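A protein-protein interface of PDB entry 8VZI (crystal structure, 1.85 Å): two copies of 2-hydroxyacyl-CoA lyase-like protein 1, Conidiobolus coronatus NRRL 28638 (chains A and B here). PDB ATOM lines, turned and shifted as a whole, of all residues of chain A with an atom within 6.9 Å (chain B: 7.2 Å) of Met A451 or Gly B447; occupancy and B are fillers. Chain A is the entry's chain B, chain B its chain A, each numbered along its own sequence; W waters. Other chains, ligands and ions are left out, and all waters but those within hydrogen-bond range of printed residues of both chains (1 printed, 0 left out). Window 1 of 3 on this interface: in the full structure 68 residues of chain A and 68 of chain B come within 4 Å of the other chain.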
ATOM      1  N   ARG A  50      11.765  16.779  19.208  1.00  0.00           N
ATOM      2  CA  ARG A  50      10.432  16.268  19.490  1.00  0.00           C
ATOM      3  C   ARG A  50       9.745  15.668  18.269  1.00  0.00           C
ATOM      4  O   ARG A  50       8.740  14.962  18.428  1.00  0.00           O
ATOM      5  CB  ARG A  50       9.552  17.377  20.085  1.00  0.00           C
ATOM      6  CG  ARG A  50      10.115  18.015  21.390  1.00  0.00           C
ATOM      7  CD  ARG A  50      10.572  16.965  22.410  1.00  0.00           C
ATOM      8  NE  ARG A  50       9.478  16.123  22.881  1.00  0.00           N
ATOM      9  CZ  ARG A  50       8.773  16.330  23.986  1.00  0.00           C
ATOM     10  NH1 ARG A  50       9.032  17.346  24.800  1.00  0.00           N
ATOM     11  NH2 ARG A  50       7.771  15.500  24.281  1.00  0.00           N
ATOM     12  N   ASN A  51      10.261  15.921  17.067  1.00  0.00           N
ATOM     13  CA  ASN A  51       9.788  15.303  15.835  1.00  0.00           C
ATOM     14  C   ASN A  51      10.975  15.271  14.882  1.00  0.00           C
ATOM     15  O   ASN A  51      11.796  16.190  14.894  1.00  0.00           O
ATOM     16  CB  ASN A  51       8.625  16.089  15.227  1.00  0.00           C
ATOM     17  CG  ASN A  51       7.884  15.306  14.151  1.00  0.00           C
ATOM     18  OD1 ASN A  51       8.420  15.046  13.061  1.00  0.00           O
ATOM     19  ND2 ASN A  51       6.639  14.925  14.450  1.00  0.00           N
ATOM     20  N   LEU A 422      11.369  26.270  14.050  1.00  0.00           N
ATOM     21  CA  LEU A 422      12.099  26.002  15.281  1.00  0.00           C
ATOM     22  C   LEU A 422      13.363  25.193  15.020  1.00  0.00           C
ATOM     23  O   LEU A 422      14.380  25.408  15.689  1.00  0.00           O
ATOM     24  CB  LEU A 422      11.183  25.310  16.298  1.00  0.00           C
ATOM     25  CG  LEU A 422      10.082  26.246  16.830  1.00  0.00           C
ATOM     26  CD1 LEU A 422       9.562  25.785  18.181  1.00  0.00           C
ATOM     27  CD2 LEU A 422      10.554  27.679  16.925  1.00  0.00           C
ATOM     28  N   PHE A 446       3.860  28.370  12.793  1.00  0.00           N
ATOM     29  CA  PHE A 446       4.330  27.996  14.128  1.00  0.00           C
ATOM     30  C   PHE A 446       3.835  26.626  14.565  1.00  0.00           C
ATOM     31  O   PHE A 446       4.585  25.860  15.183  1.00  0.00           O
ATOM     32  CB  PHE A 446       3.878  29.040  15.145  1.00  0.00           C
ATOM     33  CG  PHE A 446       4.387  28.793  16.533  1.00  0.00           C
ATOM     34  CD1 PHE A 446       5.737  28.600  16.758  1.00  0.00           C
ATOM     35  CD2 PHE A 446       3.523  28.793  17.620  1.00  0.00           C
ATOM     36  CE1 PHE A 446       6.226  28.395  18.044  1.00  0.00           C
ATOM     37  CE2 PHE A 446       4.003  28.583  18.905  1.00  0.00           C
ATOM     38  CZ  PHE A 446       5.360  28.392  19.119  1.00  0.00           C
ATOM     39  N   GLY A 447       2.567  26.305  14.271  1.00  0.00           N
ATOM     40  CA  GLY A 447       1.973  25.056  14.726  1.00  0.00           C
ATOM     41  C   GLY A 447       2.630  23.801  14.178  1.00  0.00           C
ATOM     42  O   GLY A 447       2.484  22.727  14.771  1.00  0.00           O
ATOM     43  N   PHE A 448       3.346  23.907  13.056  1.00  0.00           N
ATOM     44  CA  PHE A 448       4.033  22.746  12.494  1.00  0.00           C
ATOM     45  C   PHE A 448       5.130  22.223  13.420  1.00  0.00           C
ATOM     46  O   PHE A 448       5.381  21.013  13.471  1.00  0.00           O
ATOM     47  CB  PHE A 448       4.643  23.100  11.135  1.00  0.00           C
ATOM     48  CG  PHE A 448       3.648  23.174  10.030  1.00  0.00           C
ATOM     49  CD1 PHE A 448       2.873  24.306   9.854  1.00  0.00           C
ATOM     50  CD2 PHE A 448       3.487  22.102   9.155  1.00  0.00           C
ATOM     51  CE1 PHE A 448       1.946  24.369   8.817  1.00  0.00           C
ATOM     52  CE2 PHE A 448       2.578  22.165   8.120  1.00  0.00           C
ATOM     53  CZ  PHE A 448       1.810  23.297   7.947  1.00  0.00           C
ATOM     54  N   SER A 449       5.821  23.121  14.140  1.00  0.00           N
ATOM     55  CA  SER A 449       7.011  22.721  14.885  1.00  0.00           C
ATOM     56  C   SER A 449       7.034  23.271  16.315  1.00  0.00           C
ATOM     57  O   SER A 449       8.095  23.282  16.950  1.00  0.00           O
ATOM     58  CB  SER A 449       8.275  23.150  14.135  1.00  0.00           C
ATOM     59  OG  SER A 449       8.406  24.573  14.082  1.00  0.00           O
ATOM     60  N   ALA A 450       5.889  23.697  16.851  1.00  0.00           N
ATOM     61  CA  ALA A 450       5.891  24.471  18.096  1.00  0.00           C
ATOM     62  C   ALA A 450       6.462  23.698  19.285  1.00  0.00           C
ATOM     63  O   ALA A 450       7.055  24.306  20.186  1.00  0.00           O
ATOM     64  CB  ALA A 450       4.477  24.954  18.410  1.00  0.00           C
ATOM     65  N   MET A 451       6.300  22.372  19.330  1.00  0.00           N
ATOM     66  CA  MET A 451       6.752  21.664  20.533  1.00  0.00           C
ATOM     67  C   MET A 451       8.267  21.674  20.711  1.00  0.00           C
ATOM     68  O   MET A 451       8.741  21.341  21.806  1.00  0.00           O
ATOM     69  CB  MET A 451       6.272  20.220  20.536  1.00  0.00           C
ATOM     70  CG  MET A 451       4.789  20.110  20.706  1.00  0.00           C
ATOM     71  SD  MET A 451       4.317  20.811  22.294  1.00  0.00           S
ATOM     72  CE  MET A 451       5.156  19.703  23.424  1.00  0.00           C
ATOM     73  N   GLU A 452       9.032  22.049  19.689  1.00  0.00           N
ATOM     74  CA  GLU A 452      10.475  22.160  19.877  1.00  0.00           C
ATOM     75  C   GLU A 452      10.855  23.261  20.867  1.00  0.00           C
ATOM     76  O   GLU A 452      12.039  23.378  21.195  1.00  0.00           O
ATOM     77  CB  GLU A 452      11.194  22.397  18.535  1.00  0.00           C
ATOM     78  CG  GLU A 452      10.905  21.345  17.450  1.00  0.00           C
ATOM     79  CD  GLU A 452      11.323  19.924  17.840  1.00  0.00           C
ATOM     80  OE1 GLU A 452      12.254  19.757  18.662  1.00  0.00           O
ATOM     81  OE2 GLU A 452      10.716  18.964  17.318  1.00  0.00           O
ATOM     82  N   ILE A 453       9.905  24.056  21.373  1.00  0.00           N
ATOM     83  CA  ILE A 453      10.256  24.970  22.463  1.00  0.00           C
ATOM     84  C   ILE A 453      10.772  24.191  23.659  1.00  0.00           C
ATOM     85  O   ILE A 453      11.604  24.696  24.417  1.00  0.00           O
ATOM     86  CB  ILE A 453       9.078  25.881  22.870  1.00  0.00           C
ATOM     87  CG1 ILE A 453       7.882  25.066  23.367  1.00  0.00           C
ATOM     88  CG2 ILE A 453       8.713  26.840  21.736  1.00  0.00           C
ATOM     89  CD1 ILE A 453       6.811  25.927  24.032  1.00  0.00           C
ATOM     90  N   GLU A 454      10.314  22.953  23.850  1.00  0.00           N
ATOM     91  CA  GLU A 454      10.893  22.161  24.928  1.00  0.00           C
ATOM     92  C   GLU A 454      12.338  21.783  24.621  1.00  0.00           C
ATOM     93  O   GLU A 454      13.181  21.769  25.526  1.00  0.00           O
ATOM     94  CB  GLU A 454      10.058  20.918  25.203  1.00  0.00           C
ATOM     95  CG  GLU A 454      10.539  20.155  26.434  1.00  0.00           C
ATOM     96  CD  GLU A 454      11.618  19.145  26.090  1.00  0.00           C
ATOM     97  OE1 GLU A 454      11.663  18.718  24.918  1.00  0.00           O
ATOM     98  OE2 GLU A 454      12.416  18.780  26.979  1.00  0.00           O
ATOM     99  N   THR A 455      12.648  21.463  23.359  1.00  0.00           N
ATOM    100  CA  THR A 455      14.041  21.208  22.998  1.00  0.00           C
ATOM    101  C   THR A 455      14.897  22.436  23.286  1.00  0.00           C
ATOM    102  O   THR A 455      15.988  22.334  23.863  1.00  0.00           O
ATOM    103  CB  THR A 455      14.141  20.819  21.524  1.00  0.00           C
ATOM    104  OG1 THR A 455      13.304  19.684  21.275  1.00  0.00           O
ATOM    105  CG2 THR A 455      15.580  20.473  21.170  1.00  0.00           C
ATOM    106  N   ALA A 456      14.399  23.613  22.906  1.00  0.00           N
ATOM    107  CA  ALA A 456      15.146  24.844  23.129  1.00  0.00           C
ATOM    108  C   ALA A 456      15.376  25.090  24.619  1.00  0.00           C
ATOM    109  O   ALA A 456      16.499  25.381  25.042  1.00  0.00           O
ATOM    110  CB  ALA A 456      14.404  26.011  22.482  1.00  0.00           C
ATOM    111  N   ARG A 458      15.300  22.854  27.089  1.00  0.00           N
ATOM    112  CA  ARG A 458      16.131  21.795  27.659  1.00  0.00           C
ATOM    113  C   ARG A 458      17.610  21.981  27.307  1.00  0.00           C
ATOM    114  O   ARG A 458      18.492  21.778  28.155  1.00  0.00           O
ATOM    115  CB  ARG A 458      15.624  20.428  27.170  1.00  0.00           C
ATOM    116  CG  ARG A 458      16.617  19.279  27.347  1.00  0.00           C
ATOM    117  CD  ARG A 458      15.969  17.918  27.085  1.00  0.00           C
ATOM    118  NE  ARG A 458      14.967  17.970  26.023  1.00  0.00           N
ATOM    119  CZ  ARG A 458      15.211  17.784  24.732  1.00  0.00           C
ATOM    120  NH1 ARG A 458      16.433  17.528  24.279  1.00  0.00           N
ATOM    121  NH2 ARG A 458      14.199  17.845  23.871  1.00  0.00           N
ATOM    122  N   LEU A 502       1.979  28.842  25.731  1.00  0.00           N
ATOM    123  CA  LEU A 502       2.830  27.664  25.547  1.00  0.00           C
ATOM    124  C   LEU A 502       4.171  27.816  26.252  1.00  0.00           C
ATOM    125  O   LEU A 502       4.736  26.824  26.729  1.00  0.00           O
ATOM    126  CB  LEU A 502       3.069  27.407  24.054  1.00  0.00           C
ATOM    127  CG  LEU A 502       1.837  27.149  23.172  1.00  0.00           C
ATOM    128  CD1 LEU A 502       2.239  27.096  21.692  1.00  0.00           C
ATOM    129  CD2 LEU A 502       1.101  25.878  23.578  1.00  0.00           C
ATOM    130  N   SER A 505       4.761  26.135  29.563  1.00  0.00           N
ATOM    131  CA  SER A 505       4.984  24.693  29.637  1.00  0.00           C
ATOM    132  C   SER A 505       6.454  24.348  29.816  1.00  0.00           C
ATOM    133  O   SER A 505       6.764  23.278  30.359  1.00  0.00           O
ATOM    134  CB  SER A 505       4.458  23.995  28.383  1.00  0.00           C
ATOM    135  OG  SER A 505       5.250  24.310  27.241  1.00  0.00           O
ATOM    136  N   VAL A 506       7.355  25.233  29.392  1.00  0.00           N
ATOM    137  CA  VAL A 506       8.790  24.995  29.431  1.00  0.00           C
ATOM    138  C   VAL A 506       9.497  26.032  30.298  1.00  0.00           C
ATOM    139  O   VAL A 506      10.691  26.291  30.123  1.00  0.00           O
ATOM    140  CB  VAL A 506       9.384  24.942  28.007  1.00  0.00           C
ATOM    141  CG1 VAL A 506       8.735  23.803  27.188  1.00  0.00           C
ATOM    142  CG2 VAL A 506       9.198  26.266  27.288  1.00  0.00           C
ATOM    143  N   GLU B 389      -0.314   5.365  23.238  1.00  0.00           N
ATOM    144  CA  GLU B 389       0.915   5.567  22.485  1.00  0.00           C
ATOM    145  C   GLU B 389       2.064   5.871  23.432  1.00  0.00           C
ATOM    146  O   GLU B 389       1.905   6.631  24.379  1.00  0.00           O
ATOM    147  CB  GLU B 389       0.734   6.709  21.485  1.00  0.00           C
ATOM    148  CG  GLU B 389       1.954   7.083  20.708  1.00  0.00           C
ATOM    149  CD  GLU B 389       1.726   8.355  19.917  1.00  0.00           C
ATOM    150  OE1 GLU B 389       1.221   9.342  20.498  1.00  0.00           O
ATOM    151  OE2 GLU B 389       2.015   8.354  18.710  1.00  0.00           O
ATOM    152  N   GLY B 419       3.665   9.474  17.412  1.00  0.00           N
ATOM    153  CA  GLY B 419       3.129  10.605  16.682  1.00  0.00           C
ATOM    154  C   GLY B 419       1.729  10.406  16.151  1.00  0.00           C
ATOM    155  O   GLY B 419       1.190  11.322  15.516  1.00  0.00           O
ATOM    156  N   MET B 441      -0.854   8.856  26.630  1.00  0.00           N
ATOM    157  CA  MET B 441       0.369   9.020  25.863  1.00  0.00           C
ATOM    158  C   MET B 441       1.555   9.217  26.791  1.00  0.00           C
ATOM    159  O   MET B 441       1.455   9.916  27.812  1.00  0.00           O
ATOM    160  CB  MET B 441       0.271  10.223  24.914  1.00  0.00           C
ATOM    161  CG  MET B 441      -0.619   9.977  23.696  1.00  0.00           C
ATOM    162  SD  MET B 441      -0.942  11.490  22.763  1.00  0.00           S
ATOM    163  CE  MET B 441      -1.880  12.416  23.949  1.00  0.00           C
ATOM    164  N   GLY B 442       2.685   8.624  26.417  1.00  0.00           N
ATOM    165  CA  GLY B 442       3.939   8.989  27.043  1.00  0.00           C
ATOM    166  C   GLY B 442       4.319  10.427  26.740  1.00  0.00           C
ATOM    167  O   GLY B 442       3.866  11.023  25.759  1.00  0.00           O
ATOM    168  N   ASP B 443       5.162  10.999  27.611  1.00  0.00           N
ATOM    169  CA  ASP B 443       5.555  12.390  27.418  1.00  0.00           C
ATOM    170  C   ASP B 443       6.336  12.567  26.119  1.00  0.00           C
ATOM    171  O   ASP B 443       6.110  13.536  25.381  1.00  0.00           O
ATOM    172  CB  ASP B 443       6.341  12.934  28.627  1.00  0.00           C
ATOM    173  CG  ASP B 443       7.577  12.118  28.981  1.00  0.00           C
ATOM    174  OD1 ASP B 443       7.485  10.884  29.110  1.00  0.00           O
ATOM    175  OD2 ASP B 443       8.665  12.724  29.153  1.00  0.00           O
ATOM    176  N   SER B 444       7.230  11.626  25.792  1.00  0.00           N
ATOM    177  CA  SER B 444       7.922  11.725  24.506  1.00  0.00           C
ATOM    178  C   SER B 444       6.934  11.598  23.352  1.00  0.00           C
ATOM    179  O   SER B 444       6.927  12.425  22.429  1.00  0.00           O
ATOM    180  CB  SER B 444       9.024  10.665  24.396  1.00  0.00           C
ATOM    181  OG  SER B 444       9.537  10.590  23.065  1.00  0.00           O
ATOM    182  N   ALA B 445       6.080  10.571  23.393  1.00  0.00           N
ATOM    183  CA  ALA B 445       5.115  10.366  22.316  1.00  0.00           C
ATOM    184  C   ALA B 445       4.269  11.612  22.081  1.00  0.00           C
ATOM    185  O   ALA B 445       4.025  12.003  20.932  1.00  0.00           O
ATOM    186  CB  ALA B 445       4.215   9.169  22.645  1.00  0.00           C
ATOM    187  N   PHE B 446       3.823  12.252  23.167  1.00  0.00           N
ATOM    188  CA  PHE B 446       2.904  13.380  23.059  1.00  0.00           C
ATOM    189  C   PHE B 446       3.520  14.529  22.276  1.00  0.00           C
ATOM    190  O   PHE B 446       2.821  15.225  21.529  1.00  0.00           O
ATOM    191  CB  PHE B 446       2.482  13.835  24.470  1.00  0.00           C
ATOM    192  CG  PHE B 446       1.578  15.042  24.490  1.00  0.00           C
ATOM    193  CD1 PHE B 446       0.327  15.001  23.899  1.00  0.00           C
ATOM    194  CD2 PHE B 446       1.965  16.205  25.145  1.00  0.00           C
ATOM    195  CE1 PHE B 446      -0.522  16.110  23.933  1.00  0.00           C
ATOM    196  CE2 PHE B 446       1.122  17.314  25.189  1.00  0.00           C
ATOM    197  CZ  PHE B 446      -0.127  17.258  24.588  1.00  0.00           C
ATOM    198  N   GLY B 447       4.829  14.746  22.426  1.00  0.00           N
ATOM    199  CA  GLY B 447       5.443  15.887  21.781  1.00  0.00           C
ATOM    200  C   GLY B 447       5.495  15.784  20.268  1.00  0.00           C
ATOM    201  O   GLY B 447       5.694  16.801  19.601  1.00  0.00           O
ATOM    202  N   PHE B 448       5.317  14.584  19.712  1.00  0.00           N
ATOM    203  CA  PHE B 448       5.281  14.468  18.258  1.00  0.00           C
ATOM    204  C   PHE B 448       4.084  15.203  17.667  1.00  0.00           C
ATOM    205  O   PHE B 448       4.193  15.767  16.576  1.00  0.00           O
ATOM    206  CB  PHE B 448       5.250  13.001  17.830  1.00  0.00           C
ATOM    207  CG  PHE B 448       6.574  12.299  17.931  1.00  0.00           C
ATOM    208  CD1 PHE B 448       7.021  11.803  19.146  1.00  0.00           C
ATOM    209  CD2 PHE B 448       7.367  12.120  16.793  1.00  0.00           C
ATOM    210  CE1 PHE B 448       8.239  11.144  19.241  1.00  0.00           C
ATOM    211  CE2 PHE B 448       8.580  11.458  16.871  1.00  0.00           C
ATOM    212  CZ  PHE B 448       9.021  10.970  18.096  1.00  0.00           C
ATOM    213  N   SER B 449       2.937  15.228  18.370  1.00  0.00           N
ATOM    214  CA  SER B 449       1.706  15.723  17.763  1.00  0.00           C
ATOM    215  C   SER B 449       0.934  16.691  18.654  1.00  0.00           C
ATOM    216  O   SER B 449      -0.231  16.975  18.367  1.00  0.00           O
ATOM    217  CB  SER B 449       0.791  14.562  17.366  1.00  0.00           C
ATOM    218  OG  SER B 449       0.367  13.821  18.500  1.00  0.00           O
ATOM    219  N   ALA B 450       1.572  17.245  19.694  1.00  0.00           N
ATOM    220  CA  ALA B 450       0.840  17.962  20.734  1.00  0.00           C
ATOM    221  C   ALA B 450       0.063  19.159  20.195  1.00  0.00           C
ATOM    222  O   ALA B 450      -0.981  19.510  20.754  1.00  0.00           O
ATOM    223  CB  ALA B 450       1.806  18.414  21.831  1.00  0.00           C
ATOM    224  N   MET B 451       0.531  19.801  19.118  1.00  0.00           N
ATOM    225  CA  MET B 451      -0.157  21.028  18.710  1.00  0.00           C
ATOM    226  C   MET B 451      -1.529  20.778  18.110  1.00  0.00           C
ATOM    227  O   MET B 451      -2.285  21.744  17.930  1.00  0.00           O
ATOM    228  CB  MET B 451       0.672  21.826  17.712  1.00  0.00           C
ATOM    229  CG  MET B 451       1.858  22.507  18.338  1.00  0.00           C
ATOM    230  SD  MET B 451       1.370  23.620  19.673  1.00  0.00           S
ATOM    231  CE  MET B 451       0.367  24.809  18.790  1.00  0.00           C
ATOM    232  N   LEU B 493      14.180  14.180  28.537  1.00  0.00           N
ATOM    233  CA  LEU B 493      13.522  15.439  28.237  1.00  0.00           C
ATOM    234  C   LEU B 493      13.677  16.337  29.454  1.00  0.00           C
ATOM    235  O   LEU B 493      14.292  15.954  30.457  1.00  0.00           O
ATOM    236  CB  LEU B 493      12.053  15.205  27.878  1.00  0.00           C
ATOM    237  CG  LEU B 493      11.890  14.400  26.584  1.00  0.00           C
ATOM    238  CD1 LEU B 493      10.454  13.977  26.384  1.00  0.00           C
ATOM    239  CD2 LEU B 493      12.383  15.201  25.390  1.00  0.00           C
ATOM    240  N   THR B 497       8.346  18.861  32.646  1.00  0.00           N
ATOM    241  CA  THR B 497       7.787  19.691  31.588  1.00  0.00           C
ATOM    242  C   THR B 497       6.279  19.811  31.814  1.00  0.00           C
ATOM    243  O   THR B 497       5.605  18.823  32.107  1.00  0.00           O
ATOM    244  CB  THR B 497       8.102  19.080  30.216  1.00  0.00           C
ATOM    245  OG1 THR B 497       9.516  19.140  29.988  1.00  0.00           O
ATOM    246  CG2 THR B 497       7.407  19.847  29.107  1.00  0.00           C
ATOM    247  N   TYR B 499       3.279  19.970  30.481  1.00  0.00           N
ATOM    248  CA  TYR B 499       2.356  19.714  29.381  1.00  0.00           C
ATOM    249  C   TYR B 499       0.935  20.127  29.737  1.00  0.00           C
ATOM    250  O   TYR B 499       0.173  20.541  28.857  1.00  0.00           O
ATOM    251  CB  TYR B 499       2.400  18.239  28.992  1.00  0.00           C
ATOM    252  CG  TYR B 499       3.765  17.770  28.524  1.00  0.00           C
ATOM    253  CD1 TYR B 499       4.254  18.109  27.264  1.00  0.00           C
ATOM    254  CD2 TYR B 499       4.557  16.969  29.341  1.00  0.00           C
ATOM    255  CE1 TYR B 499       5.516  17.667  26.840  1.00  0.00           C
ATOM    256  CE2 TYR B 499       5.804  16.529  28.926  1.00  0.00           C
ATOM    257  CZ  TYR B 499       6.278  16.873  27.681  1.00  0.00           C
ATOM    258  OH  TYR B 499       7.535  16.431  27.308  1.00  0.00           O
ATOM    259  N   LEU B 502      -0.167  23.479  28.499  1.00  0.00           N
ATOM    260  CA  LEU B 502      -0.482  23.629  27.081  1.00  0.00           C
ATOM    261  C   LEU B 502      -1.981  23.753  26.860  1.00  0.00           C
ATOM    262  O   LEU B 502      -2.418  24.387  25.891  1.00  0.00           O
ATOM    263  CB  LEU B 502       0.058  22.442  26.285  1.00  0.00           C
ATOM    264  CG  LEU B 502       1.569  22.204  26.295  1.00  0.00           C
ATOM    265  CD1 LEU B 502       1.869  20.917  25.558  1.00  0.00           C
ATOM    266  CD2 LEU B 502       2.326  23.359  25.650  1.00  0.00           C
HETATM  267  O   HOH W   1       8.773  14.036  21.138  1.00  0.00           O
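The backbone carbonyl oxygen of Asp B443 lies within hydrogen-bond range of the guanidinium group of Arg A50 (2.8 Å). The backbone carbonyl oxygen (O) of Phe B448 sits at hydrogen-bond distance from the side-chain amide nitrogen (ND2) of Asn A51 (3.3 Å). NH1 of Arg A50 sits at hydrogen-bond distance from OH of Tyr B499, 3.1 Å away.
N of Arg A50 is in hydrogen-bond range of OE1 of Glu A452 (3.1 Å). The side-chain carboxylate of Glu A454 lies within salt-bridge range of the guanidinium group of Arg A50. The backbone NH (N) of Asn A51 is in hydrogen-bond range of the side-chain carboxylate (OE2) of Glu A452, at 3.1 Å. OE2 of Glu A454 lies within salt-bridge range of NE of Arg A458 (2.8 Å). The guanidinium group of Arg A458 is in hydrogen-bond range of the side-chain hydroxyl of Thr A455 (3.3 Å). The backbone carbonyl oxygen (O) of Leu A502 sits at hydrogen-bond distance from the side-chain hydroxyl (OG) of Ser A505 (2.6 Å).
Among the printed residues, merely in contact across the chains: Arg A50 with Ser B444 (3.7 Å), Arg A50 with Gly B447 (3.4 Å), Arg A50 with Phe B448 (3.5 Å), Arg A50 with Leu B493 (3.7 Å), Gly A447 with Met B451 (3.6 Å), Ala A450 with Met B451 (3.6 Å), Met A451 with Gly B447 (3.6 Å), Met A451 with Ala B450 (3.5 Å), Met A451 with Tyr B499 (3.99 Å), Glu A454 with Leu B493 (3.6 Å), Glu A454 with Thr B497 (3.8 Å), Arg A458 with Leu B493 (3.5 Å), Leu A502 with Leu B502 (3.5 Å), Ser A505 with Thr B497 (3.7 Å) and Ser A505 with Leu B502 (3.5 Å).
Of the printed residues of chain B, Met A451 touches Gly B447 (3.6 Å), Ala B450 (3.5 Å) and Tyr B499 (3.99 Å). Printed residues of chain B within 4 Å of Asn A51: Phe B448 (3.3 Å). Of the printed residues of chain A, Met B451 touches Gly A447 (3.6 Å) and Ala A450 (3.6 Å). Printed residues of chain B within 4 Å of Arg A458: Leu B493. Printed residues of chain B within 4 Å of Leu A502: Leu B502 (3.5 Å). The nearest residue of chain A that does not touch Gly B447 is Asn A51 (5.3 Å).
Of the 17 printed residues of chain B, 10 touch a printed residue of chain A. Of the 18 printed residues of chain A, 9 touch a printed residue of chain B. Printed residues of chain A that touch a printed residue of chain B: Arg A50, Asn A51, Gly A447, Ala A450, Met A451, Glu A454, Arg A458, Leu A502 and Ser A505. Hydrophobic or aromatic side chains of chain A within 4 Å of the printed part of chain B: Ala A450, Met A451 and Leu A502. Among the printed residues, 18 pairs touch across the chains. Among the printed residues, no Asp or Glu carboxylate lies within 4 Å of a Lys or Arg side-chain nitrogen of the other chain.
Gly A447 touches Met B451, and with the chains exchanged Met A451 touches Gly B447. Ala A450 touches Met B451, and with the chains exchanged Met A451 touches Ala B450. Leu A502 touches its own counterpart, Leu B502. Of the 18 pairs that touch across the chains among the printed residues, 5 have their exchanged pair printed and touching as well.
Water W1 lies within hydrogen-bond range of O of Ser B444 (2.8 Å) and NE of Arg A50 (2.8 Å).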
